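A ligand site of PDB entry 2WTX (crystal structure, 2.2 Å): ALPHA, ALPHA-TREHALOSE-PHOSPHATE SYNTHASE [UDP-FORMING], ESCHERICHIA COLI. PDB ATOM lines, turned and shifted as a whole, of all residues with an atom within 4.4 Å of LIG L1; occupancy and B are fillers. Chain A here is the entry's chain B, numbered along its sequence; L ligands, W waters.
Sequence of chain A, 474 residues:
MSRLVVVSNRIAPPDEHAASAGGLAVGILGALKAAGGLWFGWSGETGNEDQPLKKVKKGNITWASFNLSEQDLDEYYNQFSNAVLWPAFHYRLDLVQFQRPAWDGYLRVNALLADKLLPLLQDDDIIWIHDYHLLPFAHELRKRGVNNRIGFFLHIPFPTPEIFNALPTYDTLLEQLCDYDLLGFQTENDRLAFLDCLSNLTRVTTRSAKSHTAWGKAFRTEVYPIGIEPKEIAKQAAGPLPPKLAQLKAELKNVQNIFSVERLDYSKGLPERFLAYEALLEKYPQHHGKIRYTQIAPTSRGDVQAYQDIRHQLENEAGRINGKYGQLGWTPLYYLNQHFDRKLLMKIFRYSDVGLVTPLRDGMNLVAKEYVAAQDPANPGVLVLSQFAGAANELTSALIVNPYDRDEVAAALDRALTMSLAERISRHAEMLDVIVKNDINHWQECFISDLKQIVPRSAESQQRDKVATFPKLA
An oxygen (O12) of LIG L1 lies within hydrogen-bond range of the backbone NH (N) of Gly 23, at 2.6 Å.
The side-chain carboxylate of Glu 370 sits at hydrogen-bond distance from an oxygen (O3) of LIG L1 (2.6 Å).
An oxygen (O2) of LIG L1 sits at hydrogen-bond distance from the backbone NH of Phe 340, at 2.9 Å.
N2 of LIG L1 sits at hydrogen-bond distance from O of Phe 340, 2.7 Å away.
An oxygen (O10) of LIG L1 lies within salt-bridge range of the guanidinium group of Arg 263 (2.8 Å).
The backbone NH (N) of Leu 366 sits at hydrogen-bond distance from an oxygen (O7) of LIG L1, 2.9 Å away.
The side-chain amino group (NZ) of Lys 268 lies within salt-bridge range of an oxygen (O11) of LIG L1, 3.1 Å away.
N of Gly 22 sits at hydrogen-bond distance from O4 of LIG L1, at 3.2 Å.
The backbone NH (N) of Val 367 is in hydrogen-bond range of an oxygen (O8) of LIG L1, 3.3 Å away.
The guanidinium group of Arg 342 lies within hydrogen-bond range of an oxygen (O5) of LIG L1 (3.4 Å).
O11 of LG2 L2 lies within hydrogen-bond range of O of Gly 23 (3.2 Å).
O10 of LG2 L2 sits at hydrogen-bond distance from N of Asn 365.
The side-chain carboxylate (OD1) of Asp 362 lies within hydrogen-bond range of an oxygen (O9) of LG2 L2 (2.6 Å).
An oxygen (O12) of LIG L1 is in hydrogen-bond range of a nitrogen (N1) of LG2 L2 (2.5 Å).
OE1 of Glu 370 lies within salt-bridge range of NH2 of Arg 342.
NZ of Lys 268 lies within salt-bridge range of OD2 of Asp 362 (2.9 Å).
The backbone NH (N) of Val 367 lies close to the side-chain amide oxygen (OD1) of Asn 365 (3.4 Å).
ND2 of Asn 365 is in hydrogen-bond range of OD2 of Asp 362, at 2.9 Å.
CB of Ala 21 touches C4 of LIG L1 (3.6 Å).
Val 26 touches LIG L1 (CG2 to O5, 3.99 Å).
CG2 of Val 261 touches C3 of LIG L1, at 3.4 Å.
His 339 touches LIG L1 (CE1 to N2, 3.5 Å).
CD1 of Leu 345 touches N2 of LIG L1 (3.3 Å).
CA of Asn 365 touches O7 of LIG L1, 3.6 Å away.
Hydrophobic or aromatic side chains within 4 Å of LIG L1: Ala 21, Val 26, Val 261, His 339, Phe 340, Leu 345, Leu 366 and Val 367.
The nearest printed residue that does not touch LIG L1 is Pro 298 (4.03 Å).
Water W2 bridges O10 of LIG L1 (2.5 Å) and N of Arg 263 (3.0 Å).
Water W1 lies within hydrogen-bond range of O8 of LIG L1, NZ of Lys 268 and ND2 of Asn 365.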
ATOM      1  N   ALA A  21      -2.651 -17.281 -13.100  1.00  0.00           N
ATOM      2  CA  ALA A  21      -1.637 -18.230 -13.586  1.00  0.00           C
ATOM      3  C   ALA A  21      -2.105 -19.033 -14.820  1.00  0.00           C
ATOM      4  O   ALA A  21      -3.259 -19.438 -14.884  1.00  0.00           O
ATOM      5  CB  ALA A  21      -1.231 -19.177 -12.470  1.00  0.00           C
ATOM      6  N   GLY A  22      -1.188 -19.241 -15.771  1.00  0.00           N
ATOM      7  CA  GLY A  22      -1.470 -19.925 -17.049  1.00  0.00           C
ATOM      8  C   GLY A  22      -0.669 -19.374 -18.213  1.00  0.00           C
ATOM      9  O   GLY A  22      -0.606 -18.144 -18.419  1.00  0.00           O
ATOM     10  N   GLY A  23      -0.064 -20.256 -19.006  1.00  0.00           N
ATOM     11  CA  GLY A  23       0.813 -19.851 -20.107  1.00  0.00           C
ATOM     12  C   GLY A  23       0.164 -19.379 -21.399  1.00  0.00           C
ATOM     13  O   GLY A  23       0.806 -18.651 -22.172  1.00  0.00           O
ATOM     14  N   VAL A  26      -0.512 -15.420 -21.338  1.00  0.00           N
ATOM     15  CA  VAL A  26       0.778 -14.732 -21.434  1.00  0.00           C
ATOM     16  C   VAL A  26       1.368 -14.806 -22.858  1.00  0.00           C
ATOM     17  O   VAL A  26       1.892 -13.818 -23.372  1.00  0.00           O
ATOM     18  CB  VAL A  26       1.808 -15.268 -20.401  1.00  0.00           C
ATOM     19  CG1 VAL A  26       3.227 -14.923 -20.801  1.00  0.00           C
ATOM     20  CG2 VAL A  26       1.475 -14.733 -18.997  1.00  0.00           C
ATOM     21  N   VAL A 261       7.477 -22.945  -9.368  1.00  0.00           N
ATOM     22  CA  VAL A 261       6.199 -22.246  -9.403  1.00  0.00           C
ATOM     23  C   VAL A 261       5.338 -22.839 -10.522  1.00  0.00           C
ATOM     24  O   VAL A 261       5.818 -23.044 -11.628  1.00  0.00           O
ATOM     25  CB  VAL A 261       6.362 -20.673  -9.548  1.00  0.00           C
ATOM     26  CG1 VAL A 261       7.199 -20.324 -10.751  1.00  0.00           C
ATOM     27  CG2 VAL A 261       4.990 -19.969  -9.665  1.00  0.00           C
ATOM     28  N   ARG A 263       0.720 -23.802 -11.437  1.00  0.00           N
ATOM     29  CA  ARG A 263      -0.627 -24.123 -10.976  1.00  0.00           C
ATOM     30  C   ARG A 263      -0.581 -25.498 -10.307  1.00  0.00           C
ATOM     31  O   ARG A 263       0.162 -26.399 -10.749  1.00  0.00           O
ATOM     32  CB  ARG A 263      -1.625 -24.149 -12.129  1.00  0.00           C
ATOM     33  CG  ARG A 263      -1.786 -22.840 -12.894  1.00  0.00           C
ATOM     34  CD  ARG A 263      -2.763 -23.041 -14.059  1.00  0.00           C
ATOM     35  NE  ARG A 263      -2.194 -24.012 -15.010  1.00  0.00           N
ATOM     36  CZ  ARG A 263      -2.585 -25.269 -15.109  1.00  0.00           C
ATOM     37  NH1 ARG A 263      -3.570 -25.731 -14.336  1.00  0.00           N
ATOM     38  NH2 ARG A 263      -1.992 -26.084 -15.993  1.00  0.00           N
ATOM     39  N   LYS A 268       1.700 -31.557 -13.245  1.00  0.00           N
ATOM     40  CA  LYS A 268       2.964 -30.960 -12.820  1.00  0.00           C
ATOM     41  C   LYS A 268       3.834 -31.818 -11.900  1.00  0.00           C
ATOM     42  O   LYS A 268       4.908 -31.400 -11.527  1.00  0.00           O
ATOM     43  CB  LYS A 268       2.723 -29.587 -12.148  1.00  0.00           C
ATOM     44  CG  LYS A 268       1.893 -28.594 -12.983  1.00  0.00           C
ATOM     45  CD  LYS A 268       2.672 -28.036 -14.180  1.00  0.00           C
ATOM     46  CE  LYS A 268       1.756 -27.139 -15.043  1.00  0.00           C
ATOM     47  NZ  LYS A 268       2.525 -26.326 -16.038  1.00  0.00           N
ATOM     48  N   ILE A 296       5.730 -22.568  -5.062  1.00  0.00           N
ATOM     49  CA  ILE A 296       4.565 -21.725  -5.189  1.00  0.00           C
ATOM     50  C   ILE A 296       3.563 -22.463  -6.052  1.00  0.00           C
ATOM     51  O   ILE A 296       3.883 -22.838  -7.160  1.00  0.00           O
ATOM     52  CB  ILE A 296       4.950 -20.367  -5.750  1.00  0.00           C
ATOM     53  CG1 ILE A 296       5.873 -19.667  -4.729  1.00  0.00           C
ATOM     54  CG2 ILE A 296       3.695 -19.550  -6.071  1.00  0.00           C
ATOM     55  CD1 ILE A 296       6.161 -18.231  -5.031  1.00  0.00           C
ATOM     56  N   PRO A 298      -0.439 -21.955  -6.750  1.00  0.00           N
ATOM     57  CA  PRO A 298      -1.807 -21.472  -6.609  1.00  0.00           C
ATOM     58  C   PRO A 298      -2.837 -22.517  -7.044  1.00  0.00           C
ATOM     59  O   PRO A 298      -2.610 -23.257  -8.009  1.00  0.00           O
ATOM     60  CB  PRO A 298      -1.853 -20.258  -7.547  1.00  0.00           C
ATOM     61  CG  PRO A 298      -0.793 -20.596  -8.612  1.00  0.00           C
ATOM     62  CD  PRO A 298       0.305 -21.219  -7.797  1.00  0.00           C
ATOM     63  N   GLN A 338      -0.558 -20.031  -3.270  1.00  0.00           N
ATOM     64  CA  GLN A 338      -0.894 -18.636  -3.546  1.00  0.00           C
ATOM     65  C   GLN A 338      -0.401 -18.143  -4.894  1.00  0.00           C
ATOM     66  O   GLN A 338       0.664 -18.559  -5.376  1.00  0.00           O
ATOM     67  CB  GLN A 338      -0.304 -17.744  -2.446  1.00  0.00           C
ATOM     68  CG  GLN A 338      -0.891 -18.016  -1.053  1.00  0.00           C
ATOM     69  CD  GLN A 338      -0.096 -17.333   0.049  1.00  0.00           C
ATOM     70  OE1 GLN A 338       0.124 -16.116   0.002  1.00  0.00           O
ATOM     71  NE2 GLN A 338       0.347 -18.125   1.036  1.00  0.00           N
ATOM     72  N   HIS A 339      -1.157 -17.220  -5.481  1.00  0.00           N
ATOM     73  CA  HIS A 339      -0.776 -16.553  -6.718  1.00  0.00           C
ATOM     74  C   HIS A 339       0.222 -15.427  -6.429  1.00  0.00           C
ATOM     75  O   HIS A 339       0.055 -14.669  -5.489  1.00  0.00           O
ATOM     76  CB  HIS A 339      -2.000 -15.989  -7.454  1.00  0.00           C
ATOM     77  CG  HIS A 339      -1.644 -15.149  -8.637  1.00  0.00           C
ATOM     78  ND1 HIS A 339      -1.435 -15.681  -9.891  1.00  0.00           N
ATOM     79  CD2 HIS A 339      -1.416 -13.822  -8.752  1.00  0.00           C
ATOM     80  CE1 HIS A 339      -1.108 -14.719 -10.732  1.00  0.00           C
ATOM     81  NE2 HIS A 339      -1.085 -13.573 -10.064  1.00  0.00           N
ATOM     82  N   PHE A 340       1.248 -15.335  -7.271  1.00  0.00           N
ATOM     83  CA  PHE A 340       2.241 -14.251  -7.202  1.00  0.00           C
ATOM     84  C   PHE A 340       2.276 -13.479  -8.530  1.00  0.00           C
ATOM     85  O   PHE A 340       2.134 -14.071  -9.608  1.00  0.00           O
ATOM     86  CB  PHE A 340       3.627 -14.827  -6.889  1.00  0.00           C
ATOM     87  CG  PHE A 340       3.830 -15.166  -5.434  1.00  0.00           C
ATOM     88  CD1 PHE A 340       2.946 -15.995  -4.757  1.00  0.00           C
ATOM     89  CD2 PHE A 340       4.925 -14.650  -4.752  1.00  0.00           C
ATOM     90  CE1 PHE A 340       3.133 -16.303  -3.398  1.00  0.00           C
ATOM     91  CE2 PHE A 340       5.117 -14.958  -3.402  1.00  0.00           C
ATOM     92  CZ  PHE A 340       4.215 -15.774  -2.722  1.00  0.00           C
ATOM     93  N   ARG A 342       3.531 -11.863 -11.826  1.00  0.00           N
ATOM     94  CA  ARG A 342       4.559 -12.300 -12.745  1.00  0.00           C
ATOM     95  C   ARG A 342       5.863 -11.499 -12.613  1.00  0.00           C
ATOM     96  O   ARG A 342       6.951 -12.080 -12.587  1.00  0.00           O
ATOM     97  CB  ARG A 342       4.027 -12.305 -14.187  1.00  0.00           C
ATOM     98  CG  ARG A 342       4.939 -13.000 -15.204  1.00  0.00           C
ATOM     99  CD  ARG A 342       4.172 -13.478 -16.436  1.00  0.00           C
ATOM    100  NE  ARG A 342       5.043 -14.214 -17.353  1.00  0.00           N
ATOM    101  CZ  ARG A 342       5.554 -13.708 -18.477  1.00  0.00           C
ATOM    102  NH1 ARG A 342       5.274 -12.455 -18.835  1.00  0.00           N
ATOM    103  NH2 ARG A 342       6.328 -14.447 -19.253  1.00  0.00           N
ATOM    104  N   LEU A 345       7.673 -12.595  -9.607  1.00  0.00           N
ATOM    105  CA  LEU A 345       8.250 -13.916  -9.867  1.00  0.00           C
ATOM    106  C   LEU A 345       9.607 -13.869 -10.577  1.00  0.00           C
ATOM    107  O   LEU A 345      10.488 -14.649 -10.243  1.00  0.00           O
ATOM    108  CB  LEU A 345       7.284 -14.803 -10.653  1.00  0.00           C
ATOM    109  CG  LEU A 345       6.184 -15.493  -9.842  1.00  0.00           C
ATOM    110  CD1 LEU A 345       5.335 -16.332 -10.812  1.00  0.00           C
ATOM    111  CD2 LEU A 345       6.758 -16.368  -8.703  1.00  0.00           C
ATOM    112  N   MET A 346       9.746 -12.949 -11.528  1.00  0.00           N
ATOM    113  CA  MET A 346      10.975 -12.827 -12.320  1.00  0.00           C
ATOM    114  C   MET A 346      12.167 -12.434 -11.461  1.00  0.00           C
ATOM    115  O   MET A 346      13.270 -12.928 -11.671  1.00  0.00           O
ATOM    116  CB  MET A 346      10.789 -11.825 -13.466  1.00  0.00           C
ATOM    117  CG  MET A 346       9.621 -12.115 -14.408  1.00  0.00           C
ATOM    118  SD  MET A 346       9.710 -13.741 -15.184  1.00  0.00           S
ATOM    119  CE  MET A 346       8.357 -14.580 -14.321  1.00  0.00           C
ATOM    120  N   ASP A 362       3.778 -31.733 -20.113  1.00  0.00           N
ATOM    121  CA  ASP A 362       3.512 -30.326 -20.217  1.00  0.00           C
ATOM    122  C   ASP A 362       3.602 -29.928 -21.687  1.00  0.00           C
ATOM    123  O   ASP A 362       4.492 -30.339 -22.371  1.00  0.00           O
ATOM    124  CB  ASP A 362       4.482 -29.549 -19.323  1.00  0.00           C
ATOM    125  CG  ASP A 362       3.802 -28.459 -18.489  1.00  0.00           C
ATOM    126  OD1 ASP A 362       2.734 -27.978 -18.858  1.00  0.00           O
ATOM    127  OD2 ASP A 362       4.355 -28.063 -17.472  1.00  0.00           O
ATOM    128  N   ASN A 365       5.790 -25.340 -21.146  1.00  0.00           N
ATOM    129  CA  ASN A 365       6.228 -24.861 -19.846  1.00  0.00           C
ATOM    130  C   ASN A 365       7.025 -23.566 -19.998  1.00  0.00           C
ATOM    131  O   ASN A 365       8.215 -23.582 -20.178  1.00  0.00           O
ATOM    132  CB  ASN A 365       6.964 -25.908 -18.995  1.00  0.00           C
ATOM    133  CG  ASN A 365       7.075 -25.508 -17.519  1.00  0.00           C
ATOM    134  OD1 ASN A 365       7.776 -24.591 -17.181  1.00  0.00           O
ATOM    135  ND2 ASN A 365       6.379 -26.207 -16.658  1.00  0.00           N
ATOM    136  N   LEU A 366       6.327 -22.464 -19.937  1.00  0.00           N
ATOM    137  CA  LEU A 366       6.903 -21.141 -20.032  1.00  0.00           C
ATOM    138  C   LEU A 366       7.810 -20.830 -18.862  1.00  0.00           C
ATOM    139  O   LEU A 366       8.786 -20.178 -19.009  1.00  0.00           O
ATOM    140  CB  LEU A 366       5.852 -20.063 -20.209  1.00  0.00           C
ATOM    141  CG  LEU A 366       5.102 -20.055 -21.537  1.00  0.00           C
ATOM    142  CD1 LEU A 366       4.269 -18.870 -21.652  1.00  0.00           C
ATOM    143  CD2 LEU A 366       6.000 -20.186 -22.706  1.00  0.00           C
ATOM    144  N   VAL A 367       7.424 -21.268 -17.693  1.00  0.00           N
ATOM    145  CA  VAL A 367       8.227 -21.036 -16.469  1.00  0.00           C
ATOM    146  C   VAL A 367       9.675 -21.435 -16.630  1.00  0.00           C
ATOM    147  O   VAL A 367      10.568 -20.769 -16.121  1.00  0.00           O
ATOM    148  CB  VAL A 367       7.643 -21.785 -15.205  1.00  0.00           C
ATOM    149  CG1 VAL A 367       8.673 -21.891 -14.090  1.00  0.00           C
ATOM    150  CG2 VAL A 367       6.361 -21.105 -14.705  1.00  0.00           C
ATOM    151  N   GLU A 370      11.227 -18.692 -18.736  1.00  0.00           N
ATOM    152  CA  GLU A 370      11.259 -17.463 -17.967  1.00  0.00           C
ATOM    153  C   GLU A 370      12.401 -17.551 -16.995  1.00  0.00           C
ATOM    154  O   GLU A 370      13.141 -16.576 -16.814  1.00  0.00           O
ATOM    155  CB  GLU A 370       9.943 -17.205 -17.218  1.00  0.00           C
ATOM    156  CG  GLU A 370       8.755 -16.832 -18.105  1.00  0.00           C
ATOM    157  CD  GLU A 370       7.398 -16.951 -17.390  1.00  0.00           C
ATOM    158  OE1 GLU A 370       6.377 -16.719 -18.066  1.00  0.00           O
ATOM    159  OE2 GLU A 370       7.339 -17.316 -16.183  1.00  0.00           O
HETATM  160  N1  LIG L   1       2.462 -17.587 -13.047  1.00  0.00           N
HETATM  161  C1  LIG L   1       2.273 -16.380 -12.404  1.00  0.00           C
HETATM  162  N2  LIG L   1       2.020 -16.343 -11.046  1.00  0.00           N
HETATM  163  C2  LIG L   1       1.923 -17.522 -10.314  1.00  0.00           C
HETATM  164  C3  LIG L   1       2.090 -18.751 -10.959  1.00  0.00           C
HETATM  165  C4  LIG L   1       2.386 -18.750 -12.326  1.00  0.00           C
HETATM  166  O1  LIG L   1       2.362 -15.325 -13.034  1.00  0.00           O
HETATM  167  O2  LIG L   1       1.694 -17.471  -9.112  1.00  0.00           O
HETATM  168  C5  LIG L   1       2.715 -17.585 -14.515  1.00  0.00           C
HETATM  169  C6  LIG L   1       4.117 -17.977 -14.958  1.00  0.00           C
HETATM  170  O3  LIG L   1       5.048 -16.923 -14.922  1.00  0.00           O
HETATM  171  C7  LIG L   1       3.899 -18.483 -16.373  1.00  0.00           C
HETATM  172  C8  LIG L   1       2.486 -19.026 -16.342  1.00  0.00           C
HETATM  173  O4  LIG L   1       1.840 -18.485 -15.198  1.00  0.00           O
HETATM  174  O5  LIG L   1       3.889 -17.429 -17.324  1.00  0.00           O
HETATM  175  C9  LIG L   1       2.531 -20.548 -16.313  1.00  0.00           C
HETATM  176  O6  LIG L   1       2.644 -21.019 -17.646  1.00  0.00           O
HETATM  177  P1  LIG L   1       3.261 -22.465 -17.916  1.00  0.00           P
HETATM  178  O7  LIG L   1       3.490 -22.627 -19.373  1.00  0.00           O
HETATM  179  O8  LIG L   1       4.462 -22.706 -17.126  1.00  0.00           O
HETATM  180  O9  LIG L   1       2.226 -23.581 -17.357  1.00  0.00           O
HETATM  181  P2  LIG L   1       0.633 -23.569 -17.462  1.00  0.00           P
HETATM  182  O10 LIG L   1       0.049 -22.992 -16.240  1.00  0.00           O
HETATM  183  O11 LIG L   1       0.222 -24.996 -17.605  1.00  0.00           O
HETATM  184  O12 LIG L   1       0.075 -22.834 -18.624  1.00  0.00           O
HETATM  185  O1  LG2 L   2      -7.015 -21.324 -15.248  1.00  0.00           O
HETATM  186  P1  LG2 L   2      -7.126 -22.139 -16.604  1.00  0.00           P
HETATM  187  O2  LG2 L   2      -7.364 -21.041 -17.748  1.00  0.00           O
HETATM  188  O3  LG2 L   2      -8.244 -23.162 -16.588  1.00  0.00           O
HETATM  189  O4  LG2 L   2      -5.671 -22.762 -16.855  1.00  0.00           O
HETATM  190  C1  LG2 L   2      -4.519 -21.958 -17.217  1.00  0.00           C
HETATM  191  C2  LG2 L   2      -3.954 -22.368 -18.585  1.00  0.00           C
HETATM  192  C3  LG2 L   2      -3.168 -23.692 -18.446  1.00  0.00           C
HETATM  193  C4  LG2 L   2      -5.094 -22.448 -19.612  1.00  0.00           C
HETATM  194  O5  LG2 L   2      -5.719 -21.158 -19.749  1.00  0.00           O
HETATM  195  C5  LG2 L   2      -4.580 -22.946 -20.966  1.00  0.00           C
HETATM  196  O6  LG2 L   2      -5.684 -23.022 -21.862  1.00  0.00           O
HETATM  197  C6  LG2 L   2      -3.939 -24.328 -20.804  1.00  0.00           C
HETATM  198  O7  LG2 L   2      -3.480 -24.833 -22.052  1.00  0.00           O
HETATM  199  C7  LG2 L   2      -2.758 -24.323 -19.806  1.00  0.00           C
HETATM  200  N1  LG2 L   2      -1.485 -23.712 -20.343  1.00  0.00           N
HETATM  201  C8  LG2 L   2      -0.762 -24.398 -21.490  1.00  0.00           C
HETATM  202  C9  LG2 L   2      -0.068 -23.278 -22.280  1.00  0.00           C
HETATM  203  C10 LG2 L   2       0.245 -25.556 -21.127  1.00  0.00           C
HETATM  204  O8  LG2 L   2      -0.202 -26.273 -19.960  1.00  0.00           O
HETATM  205  C11 LG2 L   2       1.730 -25.123 -20.936  1.00  0.00           C
HETATM  206  O9  LG2 L   2       2.621 -26.248 -20.844  1.00  0.00           O
HETATM  207  C12 LG2 L   2       2.266 -24.302 -22.095  1.00  0.00           C
HETATM  208  O10 LG2 L   2       3.470 -23.638 -21.652  1.00  0.00           O
HETATM  209  C13 LG2 L   2       1.303 -23.211 -22.508  1.00  0.00           C
HETATM  210  C14 LG2 L   2       1.892 -22.013 -23.256  1.00  0.00           C
HETATM  211  O11 LG2 L   2       0.865 -21.347 -23.965  1.00  0.00           O
HETATM  212  O   HOH W   1       4.223 -24.353 -15.001  1.00  0.00           O
HETATM  213  O   HOH W   2       1.608 -23.362 -14.296  1.00  0.00           O
